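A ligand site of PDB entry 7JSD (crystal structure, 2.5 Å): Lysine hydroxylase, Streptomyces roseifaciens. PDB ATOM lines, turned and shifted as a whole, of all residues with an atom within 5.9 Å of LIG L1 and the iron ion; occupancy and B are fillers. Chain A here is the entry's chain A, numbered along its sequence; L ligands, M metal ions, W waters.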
ATOM      1  N   LEU A 131     -12.622 -18.053 -18.316  1.00  0.00           N
ATOM      2  CA  LEU A 131     -11.191 -18.213 -18.148  1.00  0.00           C
ATOM      3  C   LEU A 131     -10.490 -17.673 -19.383  1.00  0.00           C
ATOM      4  O   LEU A 131     -10.935 -17.928 -20.508  1.00  0.00           O
ATOM      5  CB  LEU A 131     -10.806 -19.687 -17.928  1.00  0.00           C
ATOM      6  CG  LEU A 131      -9.348 -19.961 -17.547  1.00  0.00           C
ATOM      7  CD1 LEU A 131      -9.086 -19.542 -16.112  1.00  0.00           C
ATOM      8  CD2 LEU A 131      -8.991 -21.424 -17.764  1.00  0.00           C
ATOM      9  N   THR A 133      -6.737 -17.975 -20.969  1.00  0.00           N
ATOM     10  CA  THR A 133      -5.387 -18.536 -20.950  1.00  0.00           C
ATOM     11  C   THR A 133      -4.496 -17.712 -21.860  1.00  0.00           C
ATOM     12  O   THR A 133      -4.904 -17.309 -22.951  1.00  0.00           O
ATOM     13  CB  THR A 133      -5.396 -19.993 -21.395  1.00  0.00           C
ATOM     14  OG1 THR A 133      -5.965 -20.102 -22.714  1.00  0.00           O
ATOM     15  CG2 THR A 133      -6.200 -20.851 -20.430  1.00  0.00           C
ATOM     16  N   GLN A 135      -0.641 -17.876 -23.378  1.00  0.00           N
ATOM     17  CA  GLN A 135       0.609 -18.581 -23.610  1.00  0.00           C
ATOM     18  C   GLN A 135       1.519 -17.720 -24.471  1.00  0.00           C
ATOM     19  O   GLN A 135       1.061 -17.079 -25.421  1.00  0.00           O
ATOM     20  CB  GLN A 135       0.364 -19.930 -24.282  1.00  0.00           C
ATOM     21  CG  GLN A 135      -0.725 -20.763 -23.642  1.00  0.00           C
ATOM     22  CD  GLN A 135      -0.904 -22.111 -24.296  1.00  0.00           C
ATOM     23  OE1 GLN A 135      -0.013 -22.592 -25.007  1.00  0.00           O
ATOM     24  NE2 GLN A 135      -2.057 -22.737 -24.072  1.00  0.00           N
ATOM     25  N   HIS A 142      -1.279 -26.355 -22.580  1.00  0.00           N
ATOM     26  CA  HIS A 142      -2.417 -26.721 -21.737  1.00  0.00           C
ATOM     27  C   HIS A 142      -2.599 -28.223 -21.941  1.00  0.00           C
ATOM     28  O   HIS A 142      -3.196 -28.657 -22.922  1.00  0.00           O
ATOM     29  CB  HIS A 142      -3.661 -25.921 -22.134  1.00  0.00           C
ATOM     30  CG  HIS A 142      -4.766 -25.982 -21.118  1.00  0.00           C
ATOM     31  ND1 HIS A 142      -5.697 -24.973 -20.982  1.00  0.00           N
ATOM     32  CD2 HIS A 142      -5.090 -26.916 -20.201  1.00  0.00           C
ATOM     33  CE1 HIS A 142      -6.551 -25.289 -20.029  1.00  0.00           C
ATOM     34  NE2 HIS A 142      -6.197 -26.464 -19.532  1.00  0.00           N
ATOM     35  N   HIS A 145      -6.455 -33.187 -20.762  1.00  0.00           N
ATOM     36  CA  HIS A 145      -7.394 -33.070 -19.648  1.00  0.00           C
ATOM     37  C   HIS A 145      -8.811 -33.240 -20.186  1.00  0.00           C
ATOM     38  O   HIS A 145      -9.047 -33.291 -21.392  1.00  0.00           O
ATOM     39  CB  HIS A 145      -7.257 -31.721 -18.942  1.00  0.00           C
ATOM     40  CG  HIS A 145      -7.735 -30.563 -19.765  1.00  0.00           C
ATOM     41  ND1 HIS A 145      -6.913 -29.895 -20.649  1.00  0.00           N
ATOM     42  CD2 HIS A 145      -8.946 -29.971 -19.856  1.00  0.00           C
ATOM     43  CE1 HIS A 145      -7.604 -28.928 -21.239  1.00  0.00           C
ATOM     44  NE2 HIS A 145      -8.839 -28.950 -20.767  1.00  0.00           N
ATOM     45  N   TRP A 146      -9.750 -33.339 -19.254  1.00  0.00           N
ATOM     46  CA  TRP A 146     -11.168 -33.134 -19.503  1.00  0.00           C
ATOM     47  C   TRP A 146     -11.651 -31.968 -18.648  1.00  0.00           C
ATOM     48  O   TRP A 146     -10.949 -31.489 -17.766  1.00  0.00           O
ATOM     49  CB  TRP A 146     -11.996 -34.394 -19.176  1.00  0.00           C
ATOM     50  CG  TRP A 146     -11.632 -35.618 -19.954  1.00  0.00           C
ATOM     51  CD1 TRP A 146     -12.230 -36.083 -21.091  1.00  0.00           C
ATOM     52  CD2 TRP A 146     -10.590 -36.551 -19.627  1.00  0.00           C
ATOM     53  NE1 TRP A 146     -11.614 -37.248 -21.505  1.00  0.00           N
ATOM     54  CE2 TRP A 146     -10.608 -37.555 -20.627  1.00  0.00           C
ATOM     55  CE3 TRP A 146      -9.645 -36.629 -18.605  1.00  0.00           C
ATOM     56  CZ2 TRP A 146      -9.718 -38.625 -20.617  1.00  0.00           C
ATOM     57  CZ3 TRP A 146      -8.759 -37.696 -18.605  1.00  0.00           C
ATOM     58  CH2 TRP A 146      -8.805 -38.684 -19.598  1.00  0.00           C
ATOM     59  N   ASP A 147     -12.867 -31.525 -18.931  1.00  0.00           N
ATOM     60  CA  ASP A 147     -13.519 -30.494 -18.126  1.00  0.00           C
ATOM     61  C   ASP A 147     -14.615 -31.133 -17.285  1.00  0.00           C
ATOM     62  O   ASP A 147     -15.172 -32.179 -17.639  1.00  0.00           O
ATOM     63  CB  ASP A 147     -14.098 -29.383 -19.000  1.00  0.00           C
ATOM     64  CG  ASP A 147     -13.042 -28.388 -19.463  1.00  0.00           C
ATOM     65  OD1 ASP A 147     -12.088 -28.805 -20.157  1.00  0.00           O
ATOM     66  OD2 ASP A 147     -13.169 -27.198 -19.136  1.00  0.00           O
ATOM     67  N   ALA A 152     -17.831 -26.279 -23.711  1.00  0.00           N
ATOM     68  CA  ALA A 152     -16.852 -25.193 -23.637  1.00  0.00           C
ATOM     69  C   ALA A 152     -16.962 -24.379 -24.906  1.00  0.00           C
ATOM     70  O   ALA A 152     -16.863 -24.919 -26.011  1.00  0.00           O
ATOM     71  CB  ALA A 152     -15.425 -25.733 -23.462  1.00  0.00           C
ATOM     72  N   ASN A 154     -15.146 -21.421 -26.836  1.00  0.00           N
ATOM     73  CA  ASN A 154     -13.803 -20.866 -26.801  1.00  0.00           C
ATOM     74  C   ASN A 154     -13.625 -19.827 -27.895  1.00  0.00           C
ATOM     75  O   ASN A 154     -14.120 -19.995 -29.016  1.00  0.00           O
ATOM     76  CB  ASN A 154     -12.758 -21.967 -26.947  1.00  0.00           C
ATOM     77  CG  ASN A 154     -12.863 -23.008 -25.839  1.00  0.00           C
ATOM     78  OD1 ASN A 154     -12.192 -22.918 -24.817  1.00  0.00           O
ATOM     79  ND2 ASN A 154     -13.724 -24.003 -26.048  1.00  0.00           N
ATOM     80  N   VAL A 168      -5.303 -27.175 -31.311  1.00  0.00           N
ATOM     81  CA  VAL A 168      -6.109 -27.953 -30.378  1.00  0.00           C
ATOM     82  C   VAL A 168      -6.099 -29.413 -30.831  1.00  0.00           C
ATOM     83  O   VAL A 168      -6.427 -29.716 -31.975  1.00  0.00           O
ATOM     84  CB  VAL A 168      -7.544 -27.412 -30.288  1.00  0.00           C
ATOM     85  CG1 VAL A 168      -8.400 -28.311 -29.417  1.00  0.00           C
ATOM     86  CG2 VAL A 168      -7.534 -25.995 -29.755  1.00  0.00           C
ATOM     87  N   LEU A 197      -6.127 -23.332 -35.564  1.00  0.00           N
ATOM     88  CA  LEU A 197      -6.912 -22.133 -35.305  1.00  0.00           C
ATOM     89  C   LEU A 197      -6.148 -20.894 -35.759  1.00  0.00           C
ATOM     90  O   LEU A 197      -4.919 -20.867 -35.729  1.00  0.00           O
ATOM     91  CB  LEU A 197      -7.270 -22.002 -33.822  1.00  0.00           C
ATOM     92  CG  LEU A 197      -8.259 -23.019 -33.237  1.00  0.00           C
ATOM     93  CD1 LEU A 197      -8.331 -22.875 -31.724  1.00  0.00           C
ATOM     94  CD2 LEU A 197      -9.641 -22.835 -33.848  1.00  0.00           C
ATOM     95  N   TYR A 203     -14.806 -21.945 -31.342  1.00  0.00           N
ATOM     96  CA  TYR A 203     -15.171 -23.351 -31.472  1.00  0.00           C
ATOM     97  C   TYR A 203     -15.957 -23.812 -30.255  1.00  0.00           C
ATOM     98  O   TYR A 203     -15.781 -23.302 -29.151  1.00  0.00           O
ATOM     99  CB  TYR A 203     -13.939 -24.242 -31.699  1.00  0.00           C
ATOM    100  CG  TYR A 203     -12.983 -24.394 -30.535  1.00  0.00           C
ATOM    101  CD1 TYR A 203     -13.213 -25.337 -29.536  1.00  0.00           C
ATOM    102  CD2 TYR A 203     -11.824 -23.641 -30.461  1.00  0.00           C
ATOM    103  CE1 TYR A 203     -12.328 -25.499 -28.492  1.00  0.00           C
ATOM    104  CE2 TYR A 203     -10.932 -23.796 -29.407  1.00  0.00           C
ATOM    105  CZ  TYR A 203     -11.192 -24.727 -28.425  1.00  0.00           C
ATOM    106  OH  TYR A 203     -10.315 -24.888 -27.377  1.00  0.00           O
ATOM    107  N   LEU A 205     -16.857 -27.112 -27.882  1.00  0.00           N
ATOM    108  CA  LEU A 205     -16.219 -28.356 -27.470  1.00  0.00           C
ATOM    109  C   LEU A 205     -17.122 -29.095 -26.495  1.00  0.00           C
ATOM    110  O   LEU A 205     -17.646 -28.494 -25.551  1.00  0.00           O
ATOM    111  CB  LEU A 205     -14.862 -28.090 -26.809  1.00  0.00           C
ATOM    112  CG  LEU A 205     -14.067 -29.314 -26.333  1.00  0.00           C
ATOM    113  CD1 LEU A 205     -13.531 -30.113 -27.513  1.00  0.00           C
ATOM    114  CD2 LEU A 205     -12.949 -28.892 -25.407  1.00  0.00           C
ATOM    115  N   SER A 207     -16.599 -30.829 -23.780  1.00  0.00           N
ATOM    116  CA  SER A 207     -15.353 -30.838 -23.021  1.00  0.00           C
ATOM    117  C   SER A 207     -15.310 -31.894 -21.925  1.00  0.00           C
ATOM    118  O   SER A 207     -14.231 -32.106 -21.352  1.00  0.00           O
ATOM    119  CB  SER A 207     -15.115 -29.463 -22.418  1.00  0.00           C
ATOM    120  OG  SER A 207     -16.206 -29.066 -21.603  1.00  0.00           O
ATOM    121  N   HIS A 212      -8.698 -33.332 -24.449  1.00  0.00           N
ATOM    122  CA  HIS A 212      -8.144 -32.300 -25.319  1.00  0.00           C
ATOM    123  C   HIS A 212      -6.958 -31.618 -24.669  1.00  0.00           C
ATOM    124  O   HIS A 212      -6.731 -31.724 -23.453  1.00  0.00           O
ATOM    125  CB  HIS A 212      -9.220 -31.255 -25.687  1.00  0.00           C
ATOM    126  CG  HIS A 212      -9.954 -30.711 -24.503  1.00  0.00           C
ATOM    127  ND1 HIS A 212     -10.919 -31.425 -23.832  1.00  0.00           N
ATOM    128  CD2 HIS A 212      -9.852 -29.518 -23.865  1.00  0.00           C
ATOM    129  CE1 HIS A 212     -11.386 -30.692 -22.837  1.00  0.00           C
ATOM    130  NE2 HIS A 212     -10.751 -29.532 -22.832  1.00  0.00           N
ATOM    131  N   ARG A 213      -6.198 -30.904 -25.490  1.00  0.00           N
ATOM    132  CA  ARG A 213      -5.009 -30.189 -25.057  1.00  0.00           C
ATOM    133  C   ARG A 213      -4.627 -29.203 -26.152  1.00  0.00           C
ATOM    134  O   ARG A 213      -5.202 -29.199 -27.241  1.00  0.00           O
ATOM    135  CB  ARG A 213      -3.847 -31.144 -24.776  1.00  0.00           C
ATOM    136  CG  ARG A 213      -3.154 -31.651 -26.033  1.00  0.00           C
ATOM    137  CD  ARG A 213      -1.667 -31.860 -25.802  1.00  0.00           C
ATOM    138  NE  ARG A 213      -0.983 -32.245 -27.029  1.00  0.00           N
ATOM    139  CZ  ARG A 213       0.341 -32.406 -27.132  1.00  0.00           C
ATOM    140  NH1 ARG A 213       1.113 -32.213 -26.076  1.00  0.00           N
ATOM    141  NH2 ARG A 213       0.872 -32.753 -28.293  1.00  0.00           N
ATOM    142  N   THR A 214      -3.647 -28.364 -25.851  1.00  0.00           N
ATOM    143  CA  THR A 214      -3.044 -27.461 -26.829  1.00  0.00           C
ATOM    144  C   THR A 214      -1.613 -27.910 -27.102  1.00  0.00           C
ATOM    145  O   THR A 214      -0.865 -28.193 -26.163  1.00  0.00           O
ATOM    146  CB  THR A 214      -3.079 -26.008 -26.356  1.00  0.00           C
ATOM    147  OG1 THR A 214      -2.167 -25.829 -25.261  1.00  0.00           O
ATOM    148  CG2 THR A 214      -4.480 -25.613 -25.908  1.00  0.00           C
ATOM    149  N   ARG A 224      -0.560 -16.717 -27.583  1.00  0.00           N
ATOM    150  CA  ARG A 224      -1.820 -17.438 -27.739  1.00  0.00           C
ATOM    151  C   ARG A 224      -2.742 -17.047 -26.591  1.00  0.00           C
ATOM    152  O   ARG A 224      -2.440 -17.341 -25.432  1.00  0.00           O
ATOM    153  CB  ARG A 224      -1.597 -18.944 -27.777  1.00  0.00           C
ATOM    154  CG  ARG A 224      -2.849 -19.759 -28.046  1.00  0.00           C
ATOM    155  CD  ARG A 224      -2.579 -21.251 -27.850  1.00  0.00           C
ATOM    156  NE  ARG A 224      -3.686 -22.090 -28.301  1.00  0.00           N
ATOM    157  CZ  ARG A 224      -4.722 -22.424 -27.537  1.00  0.00           C
ATOM    158  NH1 ARG A 224      -4.812 -21.980 -26.284  1.00  0.00           N
ATOM    159  NH2 ARG A 224      -5.688 -23.187 -28.024  1.00  0.00           N
ATOM    160  N   MET A 226      -6.702 -17.290 -25.270  1.00  0.00           N
ATOM    161  CA  MET A 226      -7.948 -18.029 -25.461  1.00  0.00           C
ATOM    162  C   MET A 226      -8.934 -17.674 -24.365  1.00  0.00           C
ATOM    163  O   MET A 226      -8.616 -17.768 -23.172  1.00  0.00           O
ATOM    164  CB  MET A 226      -7.695 -19.540 -25.457  1.00  0.00           C
ATOM    165  CG  MET A 226      -8.950 -20.380 -25.607  1.00  0.00           C
ATOM    166  SD  MET A 226      -9.622 -20.305 -27.278  1.00  0.00           S
ATOM    167  CE  MET A 226      -8.261 -21.013 -28.215  1.00  0.00           C
ATOM    168  N   VAL A 228     -12.128 -18.901 -22.571  1.00  0.00           N
ATOM    169  CA  VAL A 228     -12.808 -20.167 -22.354  1.00  0.00           C
ATOM    170  C   VAL A 228     -14.079 -19.907 -21.563  1.00  0.00           C
ATOM    171  O   VAL A 228     -14.027 -19.390 -20.438  1.00  0.00           O
ATOM    172  CB  VAL A 228     -11.910 -21.182 -21.641  1.00  0.00           C
ATOM    173  CG1 VAL A 228     -12.622 -22.521 -21.490  1.00  0.00           C
ATOM    174  CG2 VAL A 228     -10.595 -21.345 -22.397  1.00  0.00           C
HETATM  175  C1  LIG L   1      -9.734 -25.249 -21.007  1.00  0.00           C
HETATM  176  O1  LIG L   1      -9.598 -24.061 -20.600  1.00  0.00           O
HETATM  177  O2  LIG L   1     -10.305 -26.110 -20.279  1.00  0.00           O
HETATM  178  C2  LIG L   1      -9.200 -25.650 -22.378  1.00  0.00           C
HETATM  179  O3  LIG L   1      -9.343 -26.758 -22.758  1.00  0.00           O
HETATM  180  C3  LIG L   1      -8.484 -24.611 -23.237  1.00  0.00           C
HETATM  181  C4  LIG L   1      -8.288 -25.086 -24.680  1.00  0.00           C
HETATM  182  C5  LIG L   1      -7.769 -23.976 -25.580  1.00  0.00           C
HETATM  183  O4  LIG L   1      -7.058 -23.057 -25.117  1.00  0.00           O
HETATM  184  O5  LIG L   1      -8.055 -23.988 -26.808  1.00  0.00           O
HETATM  185  N1  LG2 L   2     -10.271 -29.049 -16.028  1.00  0.00           N
HETATM  186  C1  LG2 L   2      -9.359 -28.268 -16.859  1.00  0.00           C
HETATM  187  C2  LG2 L   2      -7.910 -28.686 -16.633  1.00  0.00           C
HETATM  188  O1  LG2 L   2      -7.005 -28.181 -17.287  1.00  0.00           O
HETATM  189  C3  LG2 L   2      -9.521 -26.764 -16.576  1.00  0.00           C
HETATM  190  C4  LG2 L   2     -10.789 -26.154 -17.147  1.00  0.00           C
HETATM  191  C5  LG2 L   2     -10.817 -24.657 -16.957  1.00  0.00           C
HETATM  192  C6  LG2 L   2     -11.775 -23.984 -17.933  1.00  0.00           C
HETATM  193  N2  LG2 L   2     -13.149 -24.545 -17.843  1.00  0.00           N
HETATM  194  O2  LG2 L   2      -7.617 -29.535 -15.792  1.00  0.00           O
HETATM  195 FE    FE M   1     -10.654 -27.842 -21.367  1.00  0.00          FE
HETATM  196  O   HOH W   1      -5.391 -22.884 -22.998  1.00  0.00           O
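The side-chain hydroxyl (OH) of Tyr 203 lies within hydrogen-bond range of an oxygen (O5) of LIG L1, 2.5 Å away. The guanidinium group (NH1) of Arg 224 lies within salt-bridge range of an oxygen (O4) of LIG L1 (2.8 Å). The side-chain carboxylate of Asp 147 lies within salt-bridge range of a nitrogen (N2) of LG2 L2, 3.0 Å away. A ring nitrogen (NE2) of His 142 sits at hydrogen-bond distance from an oxygen (O1) of LG2 L2 (2.9 Å). O of Trp 146 lies within hydrogen-bond range of N1 of LG2 L2 (3.1 Å).
CD2 of Leu 131 touches O1 of LIG L1, at 3.9 Å. OG1 of Thr 133 touches O4 of LIG L1, at 3.96 Å. CE1 of His 142 touches C1 of LIG L1, 3.3 Å away. Val 168 touches LIG L1 (CG2 to O5, 3.6 Å). Thr 214 touches LIG L1 (CG2 to C5, 3.7 Å). CE of Met 226 touches O5 of LIG L1 (3.3 Å). Val 228 touches LIG L1 (CG2 to O1, 3.4 Å). Hydrophobic or aromatic side chains that line LIG L1: Leu 131, His 142, His 145, Val 168, Tyr 203, His 212, Met 226 and Val 228. Of the 20 residues printed, 12 come within 4 Å of LIG L1. The nearest printed residue that does not touch LIG L1 is Asn 154 (4.4 Å).
The backbone NH (N) of Asp 147 is in hydrogen-bond range of the backbone carbonyl oxygen (O) of Ser 207, at 2.8 Å. O of Tyr 203 lies within hydrogen-bond range of N of Asn 154 (3.0 Å). O of Gln 135 is in hydrogen-bond range of N of Arg 224, at 2.7 Å. The backbone NH (N) of Thr 133 lies within hydrogen-bond range of the backbone carbonyl oxygen (O) of Met 226, 2.9 Å away. OG1 of Thr 214 lies within hydrogen-bond range of N of His 142, 2.9 Å away. The backbone NH (N) of Val 228 is in hydrogen-bond range of the backbone carbonyl oxygen (O) of Leu 131, 2.6 Å away. The side-chain hydroxyl (OG1) of Thr 214 lies within hydrogen-bond range of the side-chain amide nitrogen (NE2) of Gln 135.
O2 of LIG L1 binds the iron ion, at 2.1 Å. The iron ion is bound by OD1 of Asp 147. O3 of LIG L1 binds the iron ion (2.2 Å). The iron ion is bound by NE2 of His 145, 2.2 Å away. The iron ion is bound by NE2 of His 212, 2.2 Å away.
Of the 20 residues printed, 3 come within 4 Å of the iron ion.
Water W1 lies within hydrogen-bond range of O4 of LIG L1 (2.7 Å), OG1 of Thr 133 (2.9 Å), ND1 of His 142 (2.9 Å) and NH1 of Arg 224 (3.5 Å).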
